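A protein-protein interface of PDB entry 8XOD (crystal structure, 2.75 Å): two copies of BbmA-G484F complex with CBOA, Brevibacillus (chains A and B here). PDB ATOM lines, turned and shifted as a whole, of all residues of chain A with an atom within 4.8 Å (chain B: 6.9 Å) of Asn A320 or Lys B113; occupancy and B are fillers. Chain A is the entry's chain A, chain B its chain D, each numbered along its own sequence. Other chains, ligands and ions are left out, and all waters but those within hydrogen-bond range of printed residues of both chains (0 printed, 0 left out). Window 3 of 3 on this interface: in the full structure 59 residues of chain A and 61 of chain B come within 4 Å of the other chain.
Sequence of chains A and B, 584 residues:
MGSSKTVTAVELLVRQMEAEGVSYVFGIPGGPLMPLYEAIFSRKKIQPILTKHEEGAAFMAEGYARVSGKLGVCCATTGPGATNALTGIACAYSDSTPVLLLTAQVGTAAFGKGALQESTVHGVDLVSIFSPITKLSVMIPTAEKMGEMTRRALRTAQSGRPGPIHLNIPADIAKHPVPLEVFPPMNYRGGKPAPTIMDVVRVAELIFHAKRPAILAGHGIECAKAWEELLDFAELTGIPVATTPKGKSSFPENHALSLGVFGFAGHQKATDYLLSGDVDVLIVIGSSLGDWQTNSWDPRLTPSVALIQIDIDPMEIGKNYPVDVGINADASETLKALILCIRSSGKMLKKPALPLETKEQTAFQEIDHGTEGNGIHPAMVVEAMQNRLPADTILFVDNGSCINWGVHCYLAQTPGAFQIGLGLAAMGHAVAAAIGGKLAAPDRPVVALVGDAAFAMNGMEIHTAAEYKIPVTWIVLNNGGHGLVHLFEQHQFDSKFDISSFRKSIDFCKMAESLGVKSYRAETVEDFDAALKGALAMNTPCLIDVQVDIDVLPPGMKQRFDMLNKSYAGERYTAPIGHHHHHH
The backbone carbonyl oxygen of Lys B113 is in hydrogen-bond range of the side-chain amide nitrogen of Asn A320 (2.8 Å).
NE1 of Trp A297 is in hydrogen-bond range of O of Lys B113, 3.3 Å away.
OE1 of Glu B118 lies within hydrogen-bond range of N of Gly B114.
N of Gly B112 lies within hydrogen-bond range of OE2 of Glu B118 (3.0 Å).
OG of Ser A288 sits at hydrogen-bond distance from N of Gly A290, 3.3 Å away.
The indole nitrogen (NE1) of Trp A297 is in hydrogen-bond range of the backbone carbonyl oxygen (O) of Leu A289.
The side-chain amide nitrogen (ND2) of Asn A320 lies within hydrogen-bond range of the backbone carbonyl oxygen (O) of Leu A289 (2.9 Å).
CA of Gly A290 touches O of Lys B113, at 3.8 Å.
Gly B114 touches Gly A290.
Trp A297 touches Ala B110 (CH2 to CB, 3.8 Å).
CZ2 of Trp A297 touches O of Gly B114 (3.996 Å).
Gly B112 touches Lys A319 (O to CE, 3.4 Å).
Lys A319 touches Lys B113.
Lys B113 touches just these residues of chain A: Gly A290, Trp A297, Lys A319 and Asn A320.
Of the printed residues of chain A, Gly B114 touches Gly A290 and Trp A297.
Printed residues of chain B within 4 Å of Lys A319: Gly B112 (3.4 Å) and Lys B113 (3.4 Å).
Of the printed residues of chain B, Trp A297 touches Ala B110, Lys B113 and Gly B114.
Of the printed residues of chain A, Ala B110 touches Trp A297.
Tyr A321 touches none of the printed residues of chain B.
Leu A289 touches none of the printed residues of chain B.
No position is printed for both chains.
Of the 8 pairs that touch across the chains among the printed residues, none has its exchanged pair printed and touching as well.
Hydrophobic or aromatic side chains of chain B within 4 Å of the printed part of chain A: Ala B110.
Among the printed residues, no Asp or Glu carboxylate lies within 4 Å of a Lys or Arg side-chain nitrogen of the other chain.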
ATOM      1  N   SER A 288      -5.999 -26.852  14.808  1.00  0.00           N
ATOM      2  CA  SER A 288      -5.852 -27.565  16.063  1.00  0.00           C
ATOM      3  C   SER A 288      -5.928 -26.684  17.245  1.00  0.00           C
ATOM      4  O   SER A 288      -6.009 -27.144  18.333  1.00  0.00           O
ATOM      5  CB  SER A 288      -4.478 -28.184  16.108  1.00  0.00           C
ATOM      6  OG  SER A 288      -3.515 -27.187  16.317  1.00  0.00           O
ATOM      7  N   LEU A 289      -5.847 -25.412  16.996  1.00  0.00           N
ATOM      8  CA  LEU A 289      -5.867 -24.407  17.984  1.00  0.00           C
ATOM      9  C   LEU A 289      -4.778 -24.569  18.987  1.00  0.00           C
ATOM     10  O   LEU A 289      -4.987 -24.411  20.159  1.00  0.00           O
ATOM     11  CB  LEU A 289      -7.239 -24.203  18.601  1.00  0.00           C
ATOM     12  CG  LEU A 289      -8.432 -24.369  17.685  1.00  0.00           C
ATOM     13  CD1 LEU A 289      -9.586 -23.704  18.352  1.00  0.00           C
ATOM     14  CD2 LEU A 289      -8.193 -23.687  16.381  1.00  0.00           C
ATOM     15  N   GLY A 290      -3.539 -24.699  18.499  1.00  0.00           N
ATOM     16  CA  GLY A 290      -2.378 -24.777  19.350  1.00  0.00           C
ATOM     17  C   GLY A 290      -1.857 -23.381  19.599  1.00  0.00           C
ATOM     18  O   GLY A 290      -2.563 -22.383  19.422  1.00  0.00           O
ATOM     19  N   TRP A 297      -3.185 -19.258  23.363  1.00  0.00           N
ATOM     20  CA  TRP A 297      -4.486 -19.564  23.945  1.00  0.00           C
ATOM     21  C   TRP A 297      -5.051 -18.370  24.700  1.00  0.00           C
ATOM     22  O   TRP A 297      -5.431 -18.456  25.872  1.00  0.00           O
ATOM     23  CB  TRP A 297      -4.398 -20.772  24.861  1.00  0.00           C
ATOM     24  CG  TRP A 297      -3.687 -21.925  24.260  1.00  0.00           C
ATOM     25  CD1 TRP A 297      -4.199 -22.834  23.379  1.00  0.00           C
ATOM     26  CD2 TRP A 297      -2.328 -22.317  24.499  1.00  0.00           C
ATOM     27  NE1 TRP A 297      -3.243 -23.772  23.056  1.00  0.00           N
ATOM     28  CE2 TRP A 297      -2.088 -23.482  23.736  1.00  0.00           C
ATOM     29  CE3 TRP A 297      -1.295 -21.805  25.288  1.00  0.00           C
ATOM     30  CZ2 TRP A 297      -0.853 -24.140  23.738  1.00  0.00           C
ATOM     31  CZ3 TRP A 297      -0.077 -22.463  25.293  1.00  0.00           C
ATOM     32  CH2 TRP A 297       0.135 -23.616  24.517  1.00  0.00           C
ATOM     33  N   GLY A 318     -12.975 -29.101  20.791  1.00  0.00           N
ATOM     34  CA  GLY A 318     -13.075 -28.538  22.131  1.00  0.00           C
ATOM     35  C   GLY A 318     -11.877 -28.746  23.040  1.00  0.00           C
ATOM     36  O   GLY A 318     -11.991 -28.601  24.251  1.00  0.00           O
ATOM     37  N   LYS A 319     -10.713 -29.062  22.489  1.00  0.00           N
ATOM     38  CA  LYS A 319      -9.562 -29.369  23.329  1.00  0.00           C
ATOM     39  C   LYS A 319      -9.106 -28.149  24.162  1.00  0.00           C
ATOM     40  O   LYS A 319      -8.914 -28.264  25.383  1.00  0.00           O
ATOM     41  CB  LYS A 319      -8.483 -29.958  22.434  1.00  0.00           C
ATOM     42  CG  LYS A 319      -7.083 -29.755  22.866  1.00  0.00           C
ATOM     43  CD  LYS A 319      -6.215 -30.280  21.744  1.00  0.00           C
ATOM     44  CE  LYS A 319      -4.893 -29.547  21.568  1.00  0.00           C
ATOM     45  NZ  LYS A 319      -4.387 -30.105  20.261  1.00  0.00           N
ATOM     46  N   ASN A 320      -8.904 -26.970  23.536  1.00  0.00           N
ATOM     47  CA  ASN A 320      -8.444 -25.814  24.302  1.00  0.00           C
ATOM     48  C   ASN A 320      -9.477 -24.710  24.456  1.00  0.00           C
ATOM     49  O   ASN A 320      -9.234 -23.781  25.236  1.00  0.00           O
ATOM     50  CB  ASN A 320      -7.181 -25.210  23.686  1.00  0.00           C
ATOM     51  CG  ASN A 320      -6.068 -26.224  23.509  1.00  0.00           C
ATOM     52  OD1 ASN A 320      -5.702 -26.916  24.453  1.00  0.00           O
ATOM     53  ND2 ASN A 320      -5.559 -26.350  22.281  1.00  0.00           N
ATOM     54  N   TYR A 321     -10.613 -24.780  23.752  1.00  0.00           N
ATOM     55  CA  TYR A 321     -11.730 -23.847  23.886  1.00  0.00           C
ATOM     56  C   TYR A 321     -13.019 -24.659  23.874  1.00  0.00           C
ATOM     57  O   TYR A 321     -13.148 -25.610  23.089  1.00  0.00           O
ATOM     58  CB  TYR A 321     -11.765 -22.806  22.759  1.00  0.00           C
ATOM     59  CG  TYR A 321     -10.610 -21.835  22.838  1.00  0.00           C
ATOM     60  CD1 TYR A 321      -9.336 -22.207  22.392  1.00  0.00           C
ATOM     61  CD2 TYR A 321     -10.773 -20.556  23.371  1.00  0.00           C
ATOM     62  CE1 TYR A 321      -8.265 -21.337  22.462  1.00  0.00           C
ATOM     63  CE2 TYR A 321      -9.693 -19.663  23.454  1.00  0.00           C
ATOM     64  CZ  TYR A 321      -8.437 -20.066  22.991  1.00  0.00           C
ATOM     65  OH  TYR A 321      -7.342 -19.213  23.039  1.00  0.00           O
ATOM     66  N   PRO A 322     -13.978 -24.319  24.727  1.00  0.00           N
ATOM     67  CA  PRO A 322     -15.256 -25.039  24.715  1.00  0.00           C
ATOM     68  C   PRO A 322     -16.042 -24.726  23.450  1.00  0.00           C
ATOM     69  O   PRO A 322     -16.152 -23.569  23.035  1.00  0.00           O
ATOM     70  CB  PRO A 322     -15.966 -24.515  25.968  1.00  0.00           C
ATOM     71  CG  PRO A 322     -15.419 -23.130  26.151  1.00  0.00           C
ATOM     72  CD  PRO A 322     -14.012 -23.129  25.598  1.00  0.00           C
ATOM     73  N   THR B 108       5.226 -27.456  31.617  1.00  0.00           N
ATOM     74  CA  THR B 108       4.116 -28.354  31.943  1.00  0.00           C
ATOM     75  C   THR B 108       2.761 -27.681  31.715  1.00  0.00           C
ATOM     76  O   THR B 108       1.775 -28.361  31.403  1.00  0.00           O
ATOM     77  CB  THR B 108       4.239 -28.898  33.387  1.00  0.00           C
ATOM     78  OG1 THR B 108       4.251 -27.833  34.351  1.00  0.00           O
ATOM     79  CG2 THR B 108       5.503 -29.741  33.547  1.00  0.00           C
ATOM     80  N   ALA B 109       2.688 -26.355  31.890  1.00  0.00           N
ATOM     81  CA  ALA B 109       1.441 -25.607  31.718  1.00  0.00           C
ATOM     82  C   ALA B 109       0.879 -25.677  30.300  1.00  0.00           C
ATOM     83  O   ALA B 109      -0.244 -25.215  30.078  1.00  0.00           O
ATOM     84  CB  ALA B 109       1.645 -24.139  32.105  1.00  0.00           C
ATOM     85  N   ALA B 110       1.635 -26.202  29.341  1.00  0.00           N
ATOM     86  CA  ALA B 110       1.205 -26.330  27.960  1.00  0.00           C
ATOM     87  C   ALA B 110       1.017 -27.778  27.534  1.00  0.00           C
ATOM     88  O   ALA B 110       0.761 -28.025  26.349  1.00  0.00           O
ATOM     89  CB  ALA B 110       2.207 -25.642  27.028  1.00  0.00           C
ATOM     90  N   PHE B 111       1.185 -28.741  28.448  1.00  0.00           N
ATOM     91  CA  PHE B 111       0.978 -30.146  28.110  1.00  0.00           C
ATOM     92  C   PHE B 111      -0.447 -30.390  27.616  1.00  0.00           C
ATOM     93  O   PHE B 111      -1.430 -29.947  28.229  1.00  0.00           O
ATOM     94  CB  PHE B 111       1.269 -31.034  29.322  1.00  0.00           C
ATOM     95  CG  PHE B 111       2.725 -31.201  29.611  1.00  0.00           C
ATOM     96  CD1 PHE B 111       3.674 -30.464  28.919  1.00  0.00           C
ATOM     97  CD2 PHE B 111       3.157 -32.108  30.566  1.00  0.00           C
ATOM     98  CE1 PHE B 111       5.021 -30.619  29.182  1.00  0.00           C
ATOM     99  CE2 PHE B 111       4.507 -32.270  30.831  1.00  0.00           C
ATOM    100  CZ  PHE B 111       5.441 -31.522  30.133  1.00  0.00           C
ATOM    101  N   GLY B 112      -0.552 -31.152  26.522  1.00  0.00           N
ATOM    102  CA  GLY B 112      -1.821 -31.478  25.909  1.00  0.00           C
ATOM    103  C   GLY B 112      -2.480 -30.355  25.138  1.00  0.00           C
ATOM    104  O   GLY B 112      -3.502 -30.596  24.491  1.00  0.00           O
ATOM    105  N   LYS B 113      -1.920 -29.146  25.153  1.00  0.00           N
ATOM    106  CA  LYS B 113      -2.553 -27.988  24.537  1.00  0.00           C
ATOM    107  C   LYS B 113      -2.165 -27.780  23.078  1.00  0.00           C
ATOM    108  O   LYS B 113      -2.805 -26.976  22.396  1.00  0.00           O
ATOM    109  CB  LYS B 113      -2.202 -26.721  25.324  1.00  0.00           C
ATOM    110  CG  LYS B 113      -2.562 -26.769  26.788  1.00  0.00           C
ATOM    111  CD  LYS B 113      -3.075 -25.416  27.256  1.00  0.00           C
ATOM    112  CE  LYS B 113      -4.521 -25.183  26.825  1.00  0.00           C
ATOM    113  NZ  LYS B 113      -4.995 -23.837  27.257  1.00  0.00           N
ATOM    114  N   GLY B 114      -1.136 -28.464  22.585  1.00  0.00           N
ATOM    115  CA  GLY B 114      -0.628 -28.176  21.258  1.00  0.00           C
ATOM    116  C   GLY B 114       0.452 -27.118  21.310  1.00  0.00           C
ATOM    117  O   GLY B 114       0.439 -26.152  20.536  1.00  0.00           O
ATOM    118  N   ALA B 115       1.365 -27.268  22.267  1.00  0.00           N
ATOM    119  CA  ALA B 115       2.460 -26.326  22.410  1.00  0.00           C
ATOM    120  C   ALA B 115       3.390 -26.387  21.203  1.00  0.00           C
ATOM    121  O   ALA B 115       3.413 -27.360  20.440  1.00  0.00           O
ATOM    122  CB  ALA B 115       3.250 -26.604  23.685  1.00  0.00           C
ATOM    123  N   GLU B 118       5.737 -29.474  20.713  1.00  0.00           N
ATOM    124  CA  GLU B 118       5.487 -30.259  21.920  1.00  0.00           C
ATOM    125  C   GLU B 118       6.073 -31.673  21.809  1.00  0.00           C
ATOM    126  O   GLU B 118       5.828 -32.389  20.832  1.00  0.00           O
ATOM    127  CB  GLU B 118       3.979 -30.323  22.209  1.00  0.00           C
ATOM    128  CG  GLU B 118       3.635 -30.670  23.676  1.00  0.00           C
ATOM    129  CD  GLU B 118       2.129 -30.685  23.976  1.00  0.00           C
ATOM    130  OE1 GLU B 118       1.432 -29.688  23.653  1.00  0.00           O
ATOM    131  OE2 GLU B 118       1.646 -31.698  24.534  1.00  0.00           O
ATOM    132  N   HIS B 122       1.427 -36.374  23.960  1.00  0.00           N
ATOM    133  CA  HIS B 122       0.408 -35.716  23.144  1.00  0.00           C
ATOM    134  C   HIS B 122       0.951 -35.107  21.855  1.00  0.00           C
ATOM    135  O   HIS B 122       0.151 -34.746  20.979  1.00  0.00           O
ATOM    136  CB  HIS B 122      -0.290 -34.616  23.952  1.00  0.00           C
ATOM    137  CG  HIS B 122      -0.600 -35.002  25.366  1.00  0.00           C
ATOM    138  ND1 HIS B 122      -1.542 -35.955  25.688  1.00  0.00           N
ATOM    139  CD2 HIS B 122      -0.088 -34.566  26.543  1.00  0.00           C
ATOM    140  CE1 HIS B 122      -1.602 -36.085  27.002  1.00  0.00           C
ATOM    141  NE2 HIS B 122      -0.731 -35.253  27.544  1.00  0.00           N
